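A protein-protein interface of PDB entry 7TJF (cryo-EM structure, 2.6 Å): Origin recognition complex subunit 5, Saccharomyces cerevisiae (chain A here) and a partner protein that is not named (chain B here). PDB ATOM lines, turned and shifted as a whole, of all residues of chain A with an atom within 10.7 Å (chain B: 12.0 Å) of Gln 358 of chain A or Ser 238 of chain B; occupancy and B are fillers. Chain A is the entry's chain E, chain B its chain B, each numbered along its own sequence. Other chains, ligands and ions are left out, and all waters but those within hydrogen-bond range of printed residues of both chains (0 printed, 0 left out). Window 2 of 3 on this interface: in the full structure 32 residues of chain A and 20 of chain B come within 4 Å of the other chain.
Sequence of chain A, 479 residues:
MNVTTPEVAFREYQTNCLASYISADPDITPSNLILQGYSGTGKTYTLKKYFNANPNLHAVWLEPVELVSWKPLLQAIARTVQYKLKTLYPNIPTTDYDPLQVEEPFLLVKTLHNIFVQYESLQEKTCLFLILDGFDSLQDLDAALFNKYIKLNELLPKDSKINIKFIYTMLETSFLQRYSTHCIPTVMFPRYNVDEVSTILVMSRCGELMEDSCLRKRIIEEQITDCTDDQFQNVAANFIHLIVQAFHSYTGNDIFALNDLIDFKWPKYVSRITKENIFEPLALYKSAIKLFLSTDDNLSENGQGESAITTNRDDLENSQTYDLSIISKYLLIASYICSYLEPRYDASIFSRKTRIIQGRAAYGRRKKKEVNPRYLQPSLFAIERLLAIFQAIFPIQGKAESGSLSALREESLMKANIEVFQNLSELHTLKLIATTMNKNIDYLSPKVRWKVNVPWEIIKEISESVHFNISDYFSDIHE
Gln 358 of chain A touches one residue of chain B. Ser 238 of chain B touches four residues of chain A. Ile 357 of chain A touches just one residue of chain B: Ser 238 (3.0 Å). Gly 359 of chain A touches one residue of chain B. No residue of chain A comes within 4 Å of Ser 237 of chain B. Printed residues of chain A within 4 Å of Phe 239 of chain B: Lys 353, Thr 354 and Arg 355. Printed residues of chain A within 4 Å of Glu 244 of chain B: Ser 351 and Lys 353. Of the printed residues of chain B, Lys 353 of chain A touches Phe 239 (3.5 Å) and Glu 244 (3.5 Å). Of the printed residues of chain B, Ser 351 of chain A touches Glu 244. The nearest residue of chain B that does not touch Gln 358 of chain A is Ala 236 of chain B (5.3 Å). The nearest printed residue of chain B that does not touch Thr 354 of chain A is Glu 244 of chain B (6.2 Å).
The side-chain hydroxyl (OG) of Ser 238 of chain B sits at hydrogen-bond distance from the backbone carbonyl oxygen (O) of Ile 357 of chain A (3.0 Å). The side-chain carboxylate (OE1) of Glu 244 of chain B sits at hydrogen-bond distance from the side-chain hydroxyl (OG) of Ser 351 of chain A (3.0 Å). The side-chain carboxylate of Glu 244 of chain B lies within hydrogen-bond range of the backbone NH of Lys 353 of chain A (3.5 Å). OD1 of Asp 248 of chain B is in salt-bridge range of NH2 of Arg 355 of chain A, at 3.7 Å.
Phe 247 of chain B touches Ala 347 of chain A. Phe 239 of chain B touches Lys 353 of chain A. Thr 354 of chain A touches Phe 239 of chain B (O to CE1, 3.9 Å). Arg 355 of chain A touches Ser 238 of chain B (NE to OG, 3.5 Å). Arg 355 of chain A touches Phe 239 of chain B. Ser 238 of chain B touches Gln 358 of chain A. CA of Gly 359 of chain A touches OG of Ser 238 of chain B, at 3.8 Å.
OG of Ser 237 of chain B is in hydrogen-bond range of O of Phe 239 of chain B (2.8 Å). The backbone NH (N) of Ser 238 of chain B is in hydrogen-bond range of the side-chain carboxylate (OD2) of Asp 248 of chain B (2.8 Å). The side-chain carboxylate of Asp 248 of chain B sits at hydrogen-bond distance from the backbone NH of Phe 239 of chain B (3.3 Å). N of Glu 244 of chain B sits close to OG1 of Thr 242 of chain B, at 3.2 Å.
Of the 18 printed residues of chain B, 5 touch a printed residue of chain A. Hydrophobic or aromatic side chains of chain B that line the printed part of chain A: Phe 239 and Phe 247. Along chain B the printed residues that touch a printed residue of chain A span positions 238 to 248. Hydrophobic or aromatic side chains of chain A that line the printed part of chain B: Ala 347 and Ile 357. Among the printed residues, Asp or Glu carboxylates within 4 Å of a Lys or Arg side-chain nitrogen of the other chain: Arg 355 of chain A with Asp 248 of chain B.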
ATOM      1  N   ALA A 347     -16.059 -23.435  19.050  1.00  0.00           N
ATOM      2  CA  ALA A 347     -14.863 -24.082  19.582  1.00  0.00           C
ATOM      3  C   ALA A 347     -15.164 -24.991  20.768  1.00  0.00           C
ATOM      4  O   ALA A 347     -14.349 -25.859  21.092  1.00  0.00           O
ATOM      5  CB  ALA A 347     -13.832 -23.027  19.987  1.00  0.00           C
ATOM      6  N   SER A 351     -14.070 -28.115  18.069  1.00  0.00           N
ATOM      7  CA  SER A 351     -12.618 -28.135  18.197  1.00  0.00           C
ATOM      8  C   SER A 351     -12.152 -29.434  18.847  1.00  0.00           C
ATOM      9  O   SER A 351     -12.627 -29.807  19.923  1.00  0.00           O
ATOM     10  CB  SER A 351     -12.129 -26.935  19.003  1.00  0.00           C
ATOM     11  OG  SER A 351     -10.740 -27.025  19.260  1.00  0.00           O
ATOM     12  N   LYS A 353      -8.499 -30.771  17.969  1.00  0.00           N
ATOM     13  CA  LYS A 353      -7.157 -31.083  17.497  1.00  0.00           C
ATOM     14  C   LYS A 353      -6.122 -30.735  18.569  1.00  0.00           C
ATOM     15  O   LYS A 353      -6.292 -29.782  19.332  1.00  0.00           O
ATOM     16  CB  LYS A 353      -6.885 -30.345  16.174  1.00  0.00           C
ATOM     17  CG  LYS A 353      -5.491 -30.499  15.564  1.00  0.00           C
ATOM     18  CD  LYS A 353      -4.854 -29.177  15.198  1.00  0.00           C
ATOM     19  CE  LYS A 353      -5.377 -28.647  13.877  1.00  0.00           C
ATOM     20  NZ  LYS A 353      -4.341 -27.885  13.131  1.00  0.00           N
ATOM     21  N   THR A 354      -5.057 -31.542  18.626  1.00  0.00           N
ATOM     22  CA  THR A 354      -4.043 -31.457  19.673  1.00  0.00           C
ATOM     23  C   THR A 354      -3.270 -30.139  19.611  1.00  0.00           C
ATOM     24  O   THR A 354      -2.884 -29.675  18.537  1.00  0.00           O
ATOM     25  CB  THR A 354      -3.079 -32.643  19.539  1.00  0.00           C
ATOM     26  OG1 THR A 354      -3.830 -33.864  19.517  1.00  0.00           O
ATOM     27  CG2 THR A 354      -2.092 -32.707  20.698  1.00  0.00           C
ATOM     28  N   ARG A 355      -3.049 -29.539  20.782  1.00  0.00           N
ATOM     29  CA  ARG A 355      -2.398 -28.240  20.896  1.00  0.00           C
ATOM     30  C   ARG A 355      -0.899 -28.398  21.122  1.00  0.00           C
ATOM     31  O   ARG A 355      -0.471 -29.138  22.012  1.00  0.00           O
ATOM     32  CB  ARG A 355      -3.004 -27.441  22.050  1.00  0.00           C
ATOM     33  CG  ARG A 355      -4.319 -26.777  21.727  1.00  0.00           C
ATOM     34  CD  ARG A 355      -4.707 -25.737  22.776  1.00  0.00           C
ATOM     35  NE  ARG A 355      -5.811 -24.883  22.346  1.00  0.00           N
ATOM     36  CZ  ARG A 355      -7.080 -25.260  22.243  1.00  0.00           C
ATOM     37  NH1 ARG A 355      -7.482 -26.468  22.606  1.00  0.00           N
ATOM     38  NH2 ARG A 355      -7.976 -24.394  21.774  1.00  0.00           N
ATOM     39  N   ILE A 356      -0.110 -27.700  20.310  1.00  0.00           N
ATOM     40  CA  ILE A 356       1.306 -27.518  20.601  1.00  0.00           C
ATOM     41  C   ILE A 356       1.524 -26.258  21.435  1.00  0.00           C
ATOM     42  O   ILE A 356       2.401 -26.232  22.305  1.00  0.00           O
ATOM     43  CB  ILE A 356       2.112 -27.473  19.288  1.00  0.00           C
ATOM     44  CG1 ILE A 356       1.694 -28.629  18.367  1.00  0.00           C
ATOM     45  CG2 ILE A 356       3.627 -27.453  19.547  1.00  0.00           C
ATOM     46  CD1 ILE A 356       2.442 -29.941  18.600  1.00  0.00           C
ATOM     47  N   ILE A 357       0.711 -25.229  21.217  1.00  0.00           N
ATOM     48  CA  ILE A 357       0.811 -23.948  21.912  1.00  0.00           C
ATOM     49  C   ILE A 357      -0.232 -23.923  23.022  1.00  0.00           C
ATOM     50  O   ILE A 357      -1.372 -24.367  22.821  1.00  0.00           O
ATOM     51  CB  ILE A 357       0.629 -22.772  20.922  1.00  0.00           C
ATOM     52  CG1 ILE A 357       1.774 -22.665  19.893  1.00  0.00           C
ATOM     53  CG2 ILE A 357       0.481 -21.433  21.633  1.00  0.00           C
ATOM     54  CD1 ILE A 357       3.147 -23.183  20.319  1.00  0.00           C
ATOM     55  N   GLN A 358       0.171 -23.457  24.212  1.00  0.00           N
ATOM     56  CA  GLN A 358      -0.741 -23.316  25.345  1.00  0.00           C
ATOM     57  C   GLN A 358      -1.883 -22.359  25.027  1.00  0.00           C
ATOM     58  O   GLN A 358      -1.671 -21.277  24.472  1.00  0.00           O
ATOM     59  CB  GLN A 358       0.009 -22.813  26.581  1.00  0.00           C
ATOM     60  CG  GLN A 358       1.236 -23.609  26.957  1.00  0.00           C
ATOM     61  CD  GLN A 358       1.835 -23.179  28.275  1.00  0.00           C
ATOM     62  OE1 GLN A 358       1.814 -22.000  28.624  1.00  0.00           O
ATOM     63  NE2 GLN A 358       2.382 -24.134  29.014  1.00  0.00           N
ATOM     64  N   GLY A 359      -3.091 -22.765  25.389  1.00  0.00           N
ATOM     65  CA  GLY A 359      -4.267 -21.948  25.169  1.00  0.00           C
ATOM     66  C   GLY A 359      -5.486 -22.687  25.669  1.00  0.00           C
ATOM     67  O   GLY A 359      -5.415 -23.853  26.073  1.00  0.00           O
ATOM     68  N   ARG A 360      -6.613 -21.986  25.642  1.00  0.00           N
ATOM     69  CA  ARG A 360      -7.891 -22.546  26.056  1.00  0.00           C
ATOM     70  C   ARG A 360      -8.903 -22.389  24.933  1.00  0.00           C
ATOM     71  O   ARG A 360      -8.921 -21.370  24.235  1.00  0.00           O
ATOM     72  CB  ARG A 360      -8.421 -21.868  27.325  1.00  0.00           C
ATOM     73  CG  ARG A 360      -7.486 -21.942  28.518  1.00  0.00           C
ATOM     74  CD  ARG A 360      -7.686 -20.759  29.442  1.00  0.00           C
ATOM     75  NE  ARG A 360      -8.679 -21.040  30.469  1.00  0.00           N
ATOM     76  CZ  ARG A 360      -8.406 -21.561  31.656  1.00  0.00           C
ATOM     77  NH1 ARG A 360      -7.167 -21.854  32.015  1.00  0.00           N
ATOM     78  NH2 ARG A 360      -9.401 -21.791  32.508  1.00  0.00           N
ATOM     79  N   ALA A 361      -9.742 -23.404  24.761  1.00  0.00           N
ATOM     80  CA  ALA A 361     -10.866 -23.298  23.848  1.00  0.00           C
ATOM     81  C   ALA A 361     -12.031 -22.604  24.548  1.00  0.00           C
ATOM     82  O   ALA A 361     -11.916 -22.121  25.679  1.00  0.00           O
ATOM     83  CB  ALA A 361     -11.270 -24.678  23.331  1.00  0.00           C
ATOM     84  N   ALA A 362     -13.165 -22.533  23.860  1.00  0.00           N
ATOM     85  CA  ALA A 362     -14.374 -22.004  24.471  1.00  0.00           C
ATOM     86  C   ALA A 362     -14.892 -22.966  25.533  1.00  0.00           C
ATOM     87  O   ALA A 362     -14.879 -24.187  25.346  1.00  0.00           O
ATOM     88  CB  ALA A 362     -15.444 -21.764  23.406  1.00  0.00           C
ATOM     89  N   LYS B 234       0.855 -10.031  16.369  1.00  0.00           N
ATOM     90  CA  LYS B 234       0.683 -11.469  16.217  1.00  0.00           C
ATOM     91  C   LYS B 234      -0.311 -11.986  17.246  1.00  0.00           C
ATOM     92  O   LYS B 234      -0.292 -11.582  18.411  1.00  0.00           O
ATOM     93  CB  LYS B 234       2.022 -12.191  16.368  1.00  0.00           C
ATOM     94  CG  LYS B 234       2.040 -13.578  15.744  1.00  0.00           C
ATOM     95  CD  LYS B 234       2.884 -14.552  16.547  1.00  0.00           C
ATOM     96  CE  LYS B 234       3.012 -15.885  15.827  1.00  0.00           C
ATOM     97  NZ  LYS B 234       1.687 -16.437  15.423  1.00  0.00           N
ATOM     98  N   SER B 235      -1.193 -12.878  16.804  1.00  0.00           N
ATOM     99  CA  SER B 235      -2.227 -13.404  17.682  1.00  0.00           C
ATOM    100  C   SER B 235      -1.640 -14.387  18.687  1.00  0.00           C
ATOM    101  O   SER B 235      -0.692 -15.121  18.397  1.00  0.00           O
ATOM    102  CB  SER B 235      -3.323 -14.091  16.867  1.00  0.00           C
ATOM    103  OG  SER B 235      -2.864 -15.309  16.310  1.00  0.00           O
ATOM    104  N   ALA B 236      -2.220 -14.397  19.883  1.00  0.00           N
ATOM    105  CA  ALA B 236      -1.881 -15.392  20.900  1.00  0.00           C
ATOM    106  C   ALA B 236      -2.781 -16.618  20.784  1.00  0.00           C
ATOM    107  O   ALA B 236      -3.406 -17.059  21.747  1.00  0.00           O
ATOM    108  CB  ALA B 236      -1.971 -14.773  22.288  1.00  0.00           C
ATOM    109  N   SER B 237      -2.850 -17.173  19.579  1.00  0.00           N
ATOM    110  CA  SER B 237      -3.698 -18.313  19.277  1.00  0.00           C
ATOM    111  C   SER B 237      -2.837 -19.546  19.049  1.00  0.00           C
ATOM    112  O   SER B 237      -1.736 -19.454  18.500  1.00  0.00           O
ATOM    113  CB  SER B 237      -4.566 -18.042  18.044  1.00  0.00           C
ATOM    114  OG  SER B 237      -3.826 -18.219  16.849  1.00  0.00           O
ATOM    115  N   SER B 238      -3.346 -20.697  19.482  1.00  0.00           N
ATOM    116  CA  SER B 238      -2.623 -21.946  19.291  1.00  0.00           C
ATOM    117  C   SER B 238      -2.684 -22.434  17.852  1.00  0.00           C
ATOM    118  O   SER B 238      -1.805 -23.190  17.425  1.00  0.00           O
ATOM    119  CB  SER B 238      -3.172 -23.022  20.229  1.00  0.00           C
ATOM    120  OG  SER B 238      -3.359 -22.512  21.536  1.00  0.00           O
ATOM    121  N   PHE B 239      -3.696 -22.025  17.095  1.00  0.00           N
ATOM    122  CA  PHE B 239      -3.918 -22.565  15.767  1.00  0.00           C
ATOM    123  C   PHE B 239      -3.851 -21.448  14.736  1.00  0.00           C
ATOM    124  O   PHE B 239      -4.087 -20.277  15.042  1.00  0.00           O
ATOM    125  CB  PHE B 239      -5.275 -23.260  15.678  1.00  0.00           C
ATOM    126  CG  PHE B 239      -5.462 -24.350  16.683  1.00  0.00           C
ATOM    127  CD1 PHE B 239      -4.775 -25.547  16.576  1.00  0.00           C
ATOM    128  CD2 PHE B 239      -6.359 -24.182  17.725  1.00  0.00           C
ATOM    129  CE1 PHE B 239      -4.957 -26.540  17.519  1.00  0.00           C
ATOM    130  CE2 PHE B 239      -6.552 -25.177  18.658  1.00  0.00           C
ATOM    131  CZ  PHE B 239      -5.855 -26.359  18.550  1.00  0.00           C
ATOM    132  N   LEU B 240      -3.525 -21.821  13.505  1.00  0.00           N
ATOM    133  CA  LEU B 240      -3.481 -20.873  12.399  1.00  0.00           C
ATOM    134  C   LEU B 240      -4.407 -21.240  11.254  1.00  0.00           C
ATOM    135  O   LEU B 240      -5.072 -20.361  10.702  1.00  0.00           O
ATOM    136  CB  LEU B 240      -2.047 -20.746  11.863  1.00  0.00           C
ATOM    137  CG  LEU B 240      -0.964 -20.406  12.888  1.00  0.00           C
ATOM    138  CD1 LEU B 240       0.411 -20.754  12.346  1.00  0.00           C
ATOM    139  CD2 LEU B 240      -1.038 -18.943  13.283  1.00  0.00           C
ATOM    140  N   ASP B 241      -4.472 -22.512  10.885  1.00  0.00           N
ATOM    141  CA  ASP B 241      -5.181 -22.953   9.696  1.00  0.00           C
ATOM    142  C   ASP B 241      -6.457 -23.700  10.066  1.00  0.00           C
ATOM    143  O   ASP B 241      -6.729 -23.978  11.237  1.00  0.00           O
ATOM    144  CB  ASP B 241      -4.276 -23.832   8.829  1.00  0.00           C
ATOM    145  CG  ASP B 241      -3.157 -23.045   8.178  1.00  0.00           C
ATOM    146  OD1 ASP B 241      -3.292 -21.811   8.060  1.00  0.00           O
ATOM    147  OD2 ASP B 241      -2.145 -23.659   7.781  1.00  0.00           O
ATOM    148  N   THR B 242      -7.242 -24.003   9.024  1.00  0.00           N
ATOM    149  CA  THR B 242      -8.503 -24.746   9.061  1.00  0.00           C
ATOM    150  C   THR B 242      -9.556 -24.118   9.972  1.00  0.00           C
ATOM    151  O   THR B 242      -9.434 -22.958  10.394  1.00  0.00           O
ATOM    152  CB  THR B 242      -8.284 -26.214   9.473  1.00  0.00           C
ATOM    153  OG1 THR B 242      -7.953 -26.290  10.868  1.00  0.00           O
ATOM    154  CG2 THR B 242      -7.178 -26.861   8.648  1.00  0.00           C
ATOM    155  N   PHE B 243     -10.608 -24.890  10.267  1.00  0.00           N
ATOM    156  CA  PHE B 243     -11.641 -24.416  11.177  1.00  0.00           C
ATOM    157  C   PHE B 243     -11.124 -24.276  12.601  1.00  0.00           C
ATOM    158  O   PHE B 243     -11.677 -23.480  13.364  1.00  0.00           O
ATOM    159  CB  PHE B 243     -12.878 -25.331  11.120  1.00  0.00           C
ATOM    160  CG  PHE B 243     -12.659 -26.736  11.641  1.00  0.00           C
ATOM    161  CD1 PHE B 243     -12.918 -27.059  12.970  1.00  0.00           C
ATOM    162  CD2 PHE B 243     -12.247 -27.745  10.785  1.00  0.00           C
ATOM    163  CE1 PHE B 243     -12.728 -28.349  13.434  1.00  0.00           C
ATOM    164  CE2 PHE B 243     -12.061 -29.034  11.245  1.00  0.00           C
ATOM    165  CZ  PHE B 243     -12.304 -29.335  12.569  1.00  0.00           C
ATOM    166  N   GLU B 244     -10.069 -25.020  12.955  1.00  0.00           N
ATOM    167  CA  GLU B 244      -9.414 -24.850  14.248  1.00  0.00           C
ATOM    168  C   GLU B 244      -8.861 -23.438  14.397  1.00  0.00           C
ATOM    169  O   GLU B 244      -9.124 -22.757  15.393  1.00  0.00           O
ATOM    170  CB  GLU B 244      -8.290 -25.875  14.392  1.00  0.00           C
ATOM    171  CG  GLU B 244      -8.752 -27.307  14.562  1.00  0.00           C
ATOM    172  CD  GLU B 244      -9.334 -27.594  15.925  1.00  0.00           C
ATOM    173  OE1 GLU B 244      -8.899 -26.968  16.914  1.00  0.00           O
ATOM    174  OE2 GLU B 244     -10.214 -28.472  16.004  1.00  0.00           O
ATOM    175  N   GLY B 245      -8.120 -22.971  13.387  1.00  0.00           N
ATOM    176  CA  GLY B 245      -7.619 -21.608  13.394  1.00  0.00           C
ATOM    177  C   GLY B 245      -8.709 -20.565  13.278  1.00  0.00           C
ATOM    178  O   GLY B 245      -8.598 -19.483  13.869  1.00  0.00           O
ATOM    179  N   TYR B 246      -9.766 -20.869  12.516  1.00  0.00           N
ATOM    180  CA  TYR B 246     -10.898 -19.950  12.400  1.00  0.00           C
ATOM    181  C   TYR B 246     -11.591 -19.742  13.745  1.00  0.00           C
ATOM    182  O   TYR B 246     -11.893 -18.607  14.129  1.00  0.00           O
ATOM    183  CB  TYR B 246     -11.889 -20.472  11.358  1.00  0.00           C
ATOM    184  CG  TYR B 246     -13.092 -19.580  11.142  1.00  0.00           C
ATOM    185  CD1 TYR B 246     -13.011 -18.473  10.312  1.00  0.00           C
ATOM    186  CD2 TYR B 246     -14.313 -19.854  11.753  1.00  0.00           C
ATOM    187  CE1 TYR B 246     -14.104 -17.654  10.102  1.00  0.00           C
ATOM    188  CE2 TYR B 246     -15.412 -19.039  11.553  1.00  0.00           C
ATOM    189  CZ  TYR B 246     -15.303 -17.945  10.722  1.00  0.00           C
ATOM    190  OH  TYR B 246     -16.386 -17.129  10.520  1.00  0.00           O
ATOM    191  N   PHE B 247     -11.847 -20.825  14.481  1.00  0.00           N
ATOM    192  CA  PHE B 247     -12.494 -20.689  15.781  1.00  0.00           C
ATOM    193  C   PHE B 247     -11.536 -20.179  16.851  1.00  0.00           C
ATOM    194  O   PHE B 247     -11.981 -19.564  17.827  1.00  0.00           O
ATOM    195  CB  PHE B 247     -13.111 -22.018  16.224  1.00  0.00           C
ATOM    196  CG  PHE B 247     -14.180 -22.533  15.300  1.00  0.00           C
ATOM    197  CD1 PHE B 247     -15.057 -21.658  14.680  1.00  0.00           C
ATOM    198  CD2 PHE B 247     -14.318 -23.894  15.066  1.00  0.00           C
ATOM    199  CE1 PHE B 247     -16.039 -22.126  13.826  1.00  0.00           C
ATOM    200  CE2 PHE B 247     -15.300 -24.370  14.216  1.00  0.00           C
ATOM    201  CZ  PHE B 247     -16.163 -23.485  13.595  1.00  0.00           C
ATOM    202  N   ASP B 248     -10.231 -20.408  16.694  1.00  0.00           N
ATOM    203  CA  ASP B 248      -9.282 -19.973  17.709  1.00  0.00           C
ATOM    204  C   ASP B 248      -8.868 -18.517  17.553  1.00  0.00           C
ATOM    205  O   ASP B 248      -8.432 -17.907  18.533  1.00  0.00           O
ATOM    206  CB  ASP B 248      -8.044 -20.869  17.684  1.00  0.00           C
ATOM    207  CG  ASP B 248      -7.349 -20.941  19.027  1.00  0.00           C
ATOM    208  OD1 ASP B 248      -8.042 -21.154  20.044  1.00  0.00           O
ATOM    209  OD2 ASP B 248      -6.108 -20.799  19.068  1.00  0.00           O
ATOM    210  N   GLN B 249      -8.984 -17.947  16.356  1.00  0.00           N
ATOM    211  CA  GLN B 249      -8.630 -16.546  16.174  1.00  0.00           C
ATOM    212  C   GLN B 249      -9.812 -15.597  16.334  1.00  0.00           C
ATOM    213  O   GLN B 249      -9.599 -14.381  16.391  1.00  0.00           O
ATOM    214  CB  GLN B 249      -7.981 -16.345  14.801  1.00  0.00           C
ATOM    215  CG  GLN B 249      -6.524 -16.780  14.753  1.00  0.00           C
ATOM    216  CD  GLN B 249      -5.952 -16.783  13.351  1.00  0.00           C
ATOM    217  OE1 GLN B 249      -6.672 -16.982  12.377  1.00  0.00           O
ATOM    218  NE2 GLN B 249      -4.648 -16.562  13.245  1.00  0.00           N
ATOM    219  N   ARG B 250     -11.039 -16.107  16.397  1.00  0.00           N
ATOM    220  CA  ARG B 250     -12.218 -15.267  16.608  1.00  0.00           C
ATOM    221  C   ARG B 250     -12.659 -15.278  18.070  1.00  0.00           C
ATOM    222  O   ARG B 250     -13.793 -15.619  18.401  1.00  0.00           O
ATOM    223  CB  ARG B 250     -13.357 -15.706  15.696  1.00  0.00           C
ATOM    224  CG  ARG B 250     -13.080 -15.529  14.229  1.00  0.00           C
ATOM    225  CD  ARG B 250     -14.263 -15.983  13.413  1.00  0.00           C
ATOM    226  NE  ARG B 250     -15.327 -14.986  13.411  1.00  0.00           N
ATOM    227  CZ  ARG B 250     -15.492 -14.072  12.467  1.00  0.00           C
ATOM    228  NH1 ARG B 250     -14.678 -14.000  11.428  1.00  0.00           N
ATOM    229  NH2 ARG B 250     -16.496 -13.207  12.571  1.00  0.00           N
ATOM    230  N   LYS B 251     -11.754 -14.884  18.954  1.00  0.00           N
ATOM    231  CA  LYS B 251     -12.079 -14.764  20.362  1.00  0.00           C
ATOM    232  C   LYS B 251     -12.321 -13.292  20.702  1.00  0.00           C
ATOM    233  O   LYS B 251     -12.347 -12.426  19.822  1.00  0.00           O
ATOM    234  CB  LYS B 251     -10.980 -15.423  21.195  1.00  0.00           C
ATOM    235  CG  LYS B 251     -10.792 -16.890  20.819  1.00  0.00           C
ATOM    236  CD  LYS B 251     -10.233 -17.747  21.941  1.00  0.00           C
ATOM    237  CE  LYS B 251      -8.708 -17.787  21.958  1.00  0.00           C
ATOM    238  NZ  LYS B 251      -8.069 -16.530  22.430  1.00  0.00           N
